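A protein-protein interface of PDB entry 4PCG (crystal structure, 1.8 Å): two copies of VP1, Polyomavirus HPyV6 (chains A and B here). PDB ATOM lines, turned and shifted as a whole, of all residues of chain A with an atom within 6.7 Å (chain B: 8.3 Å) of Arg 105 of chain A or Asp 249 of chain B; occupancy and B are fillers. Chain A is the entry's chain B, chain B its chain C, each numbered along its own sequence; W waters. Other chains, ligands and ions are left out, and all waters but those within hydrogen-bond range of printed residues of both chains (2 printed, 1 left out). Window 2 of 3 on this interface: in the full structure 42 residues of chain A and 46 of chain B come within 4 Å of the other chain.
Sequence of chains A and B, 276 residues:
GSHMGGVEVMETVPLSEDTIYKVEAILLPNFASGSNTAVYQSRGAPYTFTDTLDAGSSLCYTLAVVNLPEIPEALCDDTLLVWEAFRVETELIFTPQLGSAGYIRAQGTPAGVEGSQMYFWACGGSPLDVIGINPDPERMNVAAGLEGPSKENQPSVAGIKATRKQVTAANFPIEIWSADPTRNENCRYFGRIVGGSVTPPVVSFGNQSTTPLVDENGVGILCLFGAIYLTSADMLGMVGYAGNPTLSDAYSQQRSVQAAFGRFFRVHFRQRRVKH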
ATOM      1  N   TYR A 103     -20.640 -22.006  31.197  1.00  0.00           N
ATOM      2  CA  TYR A 103     -20.504 -21.045  30.105  1.00  0.00           C
ATOM      3  C   TYR A 103     -21.831 -20.354  29.774  1.00  0.00           C
ATOM      4  O   TYR A 103     -22.897 -20.856  30.113  1.00  0.00           O
ATOM      5  CB  TYR A 103     -19.885 -21.701  28.887  1.00  0.00           C
ATOM      6  CG  TYR A 103     -20.727 -22.774  28.214  1.00  0.00           C
ATOM      7  CD1 TYR A 103     -20.646 -24.101  28.632  1.00  0.00           C
ATOM      8  CD2 TYR A 103     -21.592 -22.469  27.175  1.00  0.00           C
ATOM      9  CE1 TYR A 103     -21.386 -25.097  28.018  1.00  0.00           C
ATOM     10  CE2 TYR A 103     -22.342 -23.456  26.553  1.00  0.00           C
ATOM     11  CZ  TYR A 103     -22.240 -24.772  26.993  1.00  0.00           C
ATOM     12  OH  TYR A 103     -22.973 -25.762  26.417  1.00  0.00           O
ATOM     13  N   ILE A 104     -21.748 -19.182  29.158  1.00  0.00           N
ATOM     14  CA  ILE A 104     -22.941 -18.452  28.755  1.00  0.00           C
ATOM     15  C   ILE A 104     -23.139 -18.727  27.282  1.00  0.00           C
ATOM     16  O   ILE A 104     -22.384 -18.245  26.399  1.00  0.00           O
ATOM     17  CB  ILE A 104     -22.846 -16.941  29.008  1.00  0.00           C
ATOM     18  CG1 ILE A 104     -22.472 -16.654  30.456  1.00  0.00           C
ATOM     19  CG2 ILE A 104     -24.185 -16.267  28.655  1.00  0.00           C
ATOM     20  CD1 ILE A 104     -22.192 -15.185  30.741  1.00  0.00           C
ATOM     21  N   ARG A 105     -24.152 -19.533  26.985  1.00  0.00           N
ATOM     22  CA  ARG A 105     -24.341 -19.978  25.625  1.00  0.00           C
ATOM     23  C   ARG A 105     -24.532 -18.796  24.675  1.00  0.00           C
ATOM     24  O   ARG A 105     -23.941 -18.761  23.599  1.00  0.00           O
ATOM     25  CB  ARG A 105     -25.536 -20.938  25.542  1.00  0.00           C
ATOM     26  CG  ARG A 105     -25.858 -21.451  24.157  1.00  0.00           C
ATOM     27  CD  ARG A 105     -26.894 -22.567  24.238  1.00  0.00           C
ATOM     28  NE  ARG A 105     -26.263 -23.869  24.440  1.00  0.00           N
ATOM     29  CZ  ARG A 105     -26.814 -24.926  25.043  1.00  0.00           C
ATOM     30  NH1 ARG A 105     -28.040 -24.886  25.569  1.00  0.00           N
ATOM     31  NH2 ARG A 105     -26.109 -26.043  25.138  1.00  0.00           N
ATOM     32  N   ALA A 106     -25.346 -17.829  25.082  1.00  0.00           N
ATOM     33  CA  ALA A 106     -25.707 -16.729  24.190  1.00  0.00           C
ATOM     34  C   ALA A 106     -24.478 -15.905  23.812  1.00  0.00           C
ATOM     35  O   ALA A 106     -24.402 -15.400  22.710  1.00  0.00           O
ATOM     36  CB  ALA A 106     -26.754 -15.829  24.840  1.00  0.00           C
ATOM     37  N   GLN A 107     -23.532 -15.771  24.736  1.00  0.00           N
ATOM     38  CA  GLN A 107     -22.351 -14.960  24.509  1.00  0.00           C
ATOM     39  C   GLN A 107     -21.091 -15.762  24.156  1.00  0.00           C
ATOM     40  O   GLN A 107     -20.010 -15.192  24.063  1.00  0.00           O
ATOM     41  CB  GLN A 107     -22.094 -14.121  25.737  1.00  0.00           C
ATOM     42  CG  GLN A 107     -23.157 -13.075  25.985  1.00  0.00           C
ATOM     43  CD  GLN A 107     -22.758 -12.164  27.120  1.00  0.00           C
ATOM     44  OE1 GLN A 107     -22.527 -12.621  28.245  1.00  0.00           O
ATOM     45  NE2 GLN A 107     -22.632 -10.872  26.830  1.00  0.00           N
ATOM     46  N   GLY A 108     -21.212 -17.073  23.994  1.00  0.00           N
ATOM     47  CA  GLY A 108     -20.070 -17.912  23.597  1.00  0.00           C
ATOM     48  C   GLY A 108     -18.803 -17.732  24.442  1.00  0.00           C
ATOM     49  O   GLY A 108     -17.695 -17.709  23.901  1.00  0.00           O
ATOM     50  N   THR A 109     -18.956 -17.652  25.750  1.00  0.00           N
ATOM     51  CA  THR A 109     -17.816 -17.356  26.641  1.00  0.00           C
ATOM     52  C   THR A 109     -17.971 -18.006  28.022  1.00  0.00           C
ATOM     53  O   THR A 109     -19.099 -18.259  28.486  1.00  0.00           O
ATOM     54  CB  THR A 109     -17.604 -15.806  26.691  1.00  0.00           C
ATOM     55  OG1 THR A 109     -16.227 -15.489  27.020  1.00  0.00           O
ATOM     56  CG2 THR A 109     -18.590 -15.149  27.667  1.00  0.00           C
ATOM     57  N   PRO A 245     -24.080 -24.922  30.330  1.00  0.00           N
ATOM     58  CA  PRO A 245     -24.558 -23.541  30.254  1.00  0.00           C
ATOM     59  C   PRO A 245     -25.068 -23.058  31.584  1.00  0.00           C
ATOM     60  O   PRO A 245     -25.453 -23.861  32.441  1.00  0.00           O
ATOM     61  CB  PRO A 245     -25.706 -23.598  29.239  1.00  0.00           C
ATOM     62  CG  PRO A 245     -25.638 -24.926  28.607  1.00  0.00           C
ATOM     63  CD  PRO A 245     -24.901 -25.840  29.528  1.00  0.00           C
ATOM     64  N   THR A 246     -25.027 -21.744  31.766  1.00  0.00           N
ATOM     65  CA  THR A 246     -25.536 -21.105  32.949  1.00  0.00           C
ATOM     66  C   THR A 246     -26.007 -19.698  32.580  1.00  0.00           C
ATOM     67  O   THR A 246     -25.912 -19.299  31.428  1.00  0.00           O
ATOM     68  CB  THR A 246     -24.499 -21.087  34.086  1.00  0.00           C
ATOM     69  OG1 THR A 246     -25.132 -20.710  35.320  1.00  0.00           O
ATOM     70  CG2 THR A 246     -23.338 -20.105  33.775  1.00  0.00           C
ATOM     71  N   ALA A 250     -33.287 -22.053  31.613  1.00  0.00           N
ATOM     72  CA  ALA A 250     -33.108 -23.502  31.453  1.00  0.00           C
ATOM     73  C   ALA A 250     -32.106 -24.132  32.440  1.00  0.00           C
ATOM     74  O   ALA A 250     -32.253 -25.298  32.779  1.00  0.00           O
ATOM     75  CB  ALA A 250     -32.729 -23.834  30.008  1.00  0.00           C
ATOM     76  N   TYR A 251     -31.113 -23.382  32.932  1.00  0.00           N
ATOM     77  CA  TYR A 251     -30.108 -23.953  33.866  1.00  0.00           C
ATOM     78  C   TYR A 251     -30.116 -23.309  35.251  1.00  0.00           C
ATOM     79  O   TYR A 251     -29.109 -23.346  36.013  1.00  0.00           O
ATOM     80  CB  TYR A 251     -28.713 -23.905  33.227  1.00  0.00           C
ATOM     81  CG  TYR A 251     -28.602 -24.956  32.172  1.00  0.00           C
ATOM     82  CD1 TYR A 251     -29.085 -24.727  30.877  1.00  0.00           C
ATOM     83  CD2 TYR A 251     -28.091 -26.221  32.478  1.00  0.00           C
ATOM     84  CE1 TYR A 251     -29.020 -25.713  29.902  1.00  0.00           C
ATOM     85  CE2 TYR A 251     -28.048 -27.222  31.506  1.00  0.00           C
ATOM     86  CZ  TYR A 251     -28.495 -26.956  30.228  1.00  0.00           C
ATOM     87  OH  TYR A 251     -28.443 -27.927  29.259  1.00  0.00           O
ATOM     88  N   PHE B  49     -15.314 -25.419  26.315  1.00  0.00           N
ATOM     89  CA  PHE B  49     -16.273 -25.330  27.415  1.00  0.00           C
ATOM     90  C   PHE B  49     -16.548 -26.704  28.027  1.00  0.00           C
ATOM     91  O   PHE B  49     -17.623 -26.926  28.580  1.00  0.00           O
ATOM     92  CB  PHE B  49     -17.585 -24.670  26.933  1.00  0.00           C
ATOM     93  CG  PHE B  49     -17.419 -23.259  26.388  1.00  0.00           C
ATOM     94  CD1 PHE B  49     -16.246 -22.521  26.598  1.00  0.00           C
ATOM     95  CD2 PHE B  49     -18.461 -22.657  25.690  1.00  0.00           C
ATOM     96  CE1 PHE B  49     -16.116 -21.231  26.103  1.00  0.00           C
ATOM     97  CE2 PHE B  49     -18.335 -21.362  25.196  1.00  0.00           C
ATOM     98  CZ  PHE B  49     -17.160 -20.653  25.405  1.00  0.00           C
ATOM     99  N   THR B 246     -17.235 -12.704  17.333  1.00  0.00           N
ATOM    100  CA  THR B 246     -17.025 -13.369  18.581  1.00  0.00           C
ATOM    101  C   THR B 246     -18.126 -12.953  19.577  1.00  0.00           C
ATOM    102  O   THR B 246     -19.021 -12.187  19.238  1.00  0.00           O
ATOM    103  CB  THR B 246     -15.620 -13.077  19.123  1.00  0.00           C
ATOM    104  OG1 THR B 246     -15.346 -13.905  20.270  1.00  0.00           O
ATOM    105  CG2 THR B 246     -15.457 -11.602  19.500  1.00  0.00           C
ATOM    106  N   LEU B 247     -18.060 -13.523  20.774  1.00  0.00           N
ATOM    107  CA  LEU B 247     -19.069 -13.306  21.801  1.00  0.00           C
ATOM    108  C   LEU B 247     -20.425 -13.776  21.317  1.00  0.00           C
ATOM    109  O   LEU B 247     -21.435 -13.092  21.508  1.00  0.00           O
ATOM    110  CB  LEU B 247     -19.104 -11.831  22.210  1.00  0.00           C
ATOM    111  CG  LEU B 247     -19.571 -11.598  23.643  1.00  0.00           C
ATOM    112  CD1 LEU B 247     -18.524 -12.119  24.619  1.00  0.00           C
ATOM    113  CD2 LEU B 247     -19.887 -10.122  23.889  1.00  0.00           C
ATOM    114  N   SER B 248     -20.434 -14.946  20.666  1.00  0.00           N
ATOM    115  CA  SER B 248     -21.641 -15.630  20.262  1.00  0.00           C
ATOM    116  C   SER B 248     -21.455 -17.157  20.308  1.00  0.00           C
ATOM    117  O   SER B 248     -20.330 -17.652  20.253  1.00  0.00           O
ATOM    118  CB  SER B 248     -22.017 -15.247  18.817  1.00  0.00           C
ATOM    119  OG  SER B 248     -20.993 -15.662  17.913  1.00  0.00           O
ATOM    120  N   ASP B 249     -22.562 -17.895  20.355  1.00  0.00           N
ATOM    121  CA  ASP B 249     -22.500 -19.380  20.368  1.00  0.00           C
ATOM    122  C   ASP B 249     -21.777 -19.886  19.123  1.00  0.00           C
ATOM    123  O   ASP B 249     -20.892 -20.743  19.205  1.00  0.00           O
ATOM    124  CB  ASP B 249     -23.907 -19.998  20.451  1.00  0.00           C
ATOM    125  CG  ASP B 249     -23.903 -21.461  20.958  1.00  0.00           C
ATOM    126  OD1 ASP B 249     -22.873 -21.953  21.484  1.00  0.00           O
ATOM    127  OD2 ASP B 249     -24.961 -22.122  20.847  1.00  0.00           O
ATOM    128  N   ALA B 250     -22.138 -19.306  17.981  1.00  0.00           N
ATOM    129  CA  ALA B 250     -21.601 -19.700  16.687  1.00  0.00           C
ATOM    130  C   ALA B 250     -20.080 -19.661  16.613  1.00  0.00           C
ATOM    131  O   ALA B 250     -19.477 -20.416  15.835  1.00  0.00           O
ATOM    132  CB  ALA B 250     -22.197 -18.817  15.601  1.00  0.00           C
ATOM    133  N   TYR B 251     -19.457 -18.779  17.399  1.00  0.00           N
ATOM    134  CA  TYR B 251     -18.001 -18.628  17.377  1.00  0.00           C
ATOM    135  C   TYR B 251     -17.319 -18.945  18.687  1.00  0.00           C
ATOM    136  O   TYR B 251     -16.175 -18.525  18.920  1.00  0.00           O
ATOM    137  CB  TYR B 251     -17.636 -17.228  16.865  1.00  0.00           C
ATOM    138  CG  TYR B 251     -17.843 -17.169  15.391  1.00  0.00           C
ATOM    139  CD1 TYR B 251     -19.106 -16.938  14.866  1.00  0.00           C
ATOM    140  CD2 TYR B 251     -16.792 -17.431  14.510  1.00  0.00           C
ATOM    141  CE1 TYR B 251     -19.325 -16.933  13.500  1.00  0.00           C
ATOM    142  CE2 TYR B 251     -16.999 -17.429  13.143  1.00  0.00           C
ATOM    143  CZ  TYR B 251     -18.263 -17.177  12.653  1.00  0.00           C
ATOM    144  OH  TYR B 251     -18.482 -17.154  11.325  1.00  0.00           O
ATOM    145  N   SER B 252     -18.001 -19.719  19.527  1.00  0.00           N
ATOM    146  CA  SER B 252     -17.466 -20.064  20.843  1.00  0.00           C
ATOM    147  C   SER B 252     -16.219 -20.932  20.732  1.00  0.00           C
ATOM    148  O   SER B 252     -15.339 -20.873  21.570  1.00  0.00           O
ATOM    149  CB  SER B 252     -18.536 -20.790  21.671  1.00  0.00           C
ATOM    150  OG  SER B 252     -18.960 -21.972  21.033  1.00  0.00           O
ATOM    151  N   GLN B 253     -16.152 -21.745  19.678  1.00  0.00           N
ATOM    152  CA  GLN B 253     -14.949 -22.555  19.423  1.00  0.00           C
ATOM    153  C   GLN B 253     -13.636 -21.757  19.173  1.00  0.00           C
ATOM    154  O   GLN B 253     -12.561 -22.352  19.109  1.00  0.00           O
ATOM    155  CB  GLN B 253     -15.207 -23.592  18.304  1.00  0.00           C
ATOM    156  CG  GLN B 253     -15.204 -23.078  16.862  1.00  0.00           C
ATOM    157  CD  GLN B 253     -16.333 -22.110  16.508  1.00  0.00           C
ATOM    158  OE1 GLN B 253     -16.158 -21.257  15.636  1.00  0.00           O
ATOM    159  NE2 GLN B 253     -17.493 -22.244  17.159  1.00  0.00           N
ATOM    160  N   GLN B 254     -13.715 -20.431  19.049  1.00  0.00           N
ATOM    161  CA  GLN B 254     -12.523 -19.618  18.804  1.00  0.00           C
ATOM    162  C   GLN B 254     -12.136 -18.732  19.983  1.00  0.00           C
ATOM    163  O   GLN B 254     -11.112 -18.082  19.957  1.00  0.00           O
ATOM    164  CB  GLN B 254     -12.711 -18.795  17.530  1.00  0.00           C
ATOM    165  CG  GLN B 254     -12.711 -19.670  16.271  1.00  0.00           C
ATOM    166  CD  GLN B 254     -13.105 -18.912  15.010  1.00  0.00           C
ATOM    167  OE1 GLN B 254     -13.273 -17.689  15.014  1.00  0.00           O
ATOM    168  NE2 GLN B 254     -13.238 -19.639  13.917  1.00  0.00           N
HETATM  169  O   HOH W   1     -25.256 -16.725  20.473  1.00  0.00           O
HETATM  170  O   HOH W   2     -21.402 -21.082  23.594  1.00  0.00           O
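Arg 105 of chain A touches just one residue of chain B: Asp 249 (3.4 Å).
Ala 106 of chain A touches just these residues of chain B: Leu 247 (3.9 Å), Ser 248 (3.7 Å) and Asp 249 (3.9 Å).
Of the printed residues of chain B, Gln 107 of chain A touches Leu 247 and Ser 248.
Printed residues of chain B within 4 Å of Gly 108 of chain A: Phe 49, Ser 248, Asp 249 and Ser 252.
Pro 245 of chain A touches none of the printed residues of chain B.
Of the printed residues of chain A, Phe 49 of chain B touches Tyr 103 (3.4 Å), Gly 108 (3.3 Å) and Thr 109 (3.5 Å).
Printed residues of chain A within 4 Å of Leu 247 of chain B: Ala 106 and Gln 107.
Printed residues of chain A within 4 Å of Ser 252 of chain B: Gly 108 (3.8 Å).
The nearest residue of chain B that does not touch Arg 105 of chain A is Ser 248 of chain B (4.4 Å).
Phe 49 of chain B touches Tyr 103 of chain A.
Arg 105 of chain A touches Asp 249 of chain B (O to CB, 3.4 Å).
Ala 106 of chain A touches Leu 247 of chain B (O to O, 3.9 Å).
Ser 248 of chain B touches Ala 106 of chain A.
Ala 106 of chain A touches Asp 249 of chain B (O to N, 3.9 Å).
Gln 107 of chain A touches Leu 247 of chain B.
Gly 108 of chain A touches Ser 248 of chain B.
Gly 108 of chain A touches Asp 249 of chain B (N to N, 3.97 Å).
Gly 108 of chain A touches Ser 252 of chain B.
Phe 49 of chain B touches Thr 109 of chain A.
Water W2 lies within hydrogen-bond range of OD1 of Asp 249 of chain B (2.7 Å) and O of Arg 105 of chain A (3.4 Å).
Water W1 lies within hydrogen-bond range of the backbone carbonyl oxygen (O) of Ala 106 of chain A (2.7 Å) and the backbone NH (N) of Asp 249 of chain B (2.9 Å).
The backbone NH of Ser 248 of chain B lies within hydrogen-bond range of the backbone carbonyl oxygen of Gln 107 of chain A (3.4 Å).
The side-chain hydroxyl of Tyr 103 of chain A lies within hydrogen-bond range of the guanidinium group of Arg 105 of chain A (3.4 Å).
OG of Ser 252 of chain B lies within hydrogen-bond range of O of Asp 249 of chain B.
N of Thr 246 of chain A sits at hydrogen-bond distance from O of Tyr 103 of chain A (2.8 Å).
N of Ile 104 of chain A is in hydrogen-bond range of O of Thr 109 of chain A, 2.9 Å away.
Printed residues of chain A that touch a printed residue of chain B: Tyr 103, Arg 105, Ala 106, Gln 107, Gly 108 and Thr 109.
Hydrophobic or aromatic side chains of chain B that line the printed part of chain A: Phe 49 and Leu 247.
Among the printed residues, 12 pairs touch across the chains.
Among the printed residues, no Asp or Glu carboxylate lies within 4 Å of a Lys or Arg side-chain nitrogen of the other chain.
Positions printed for both chains: 246, 250 and 251.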
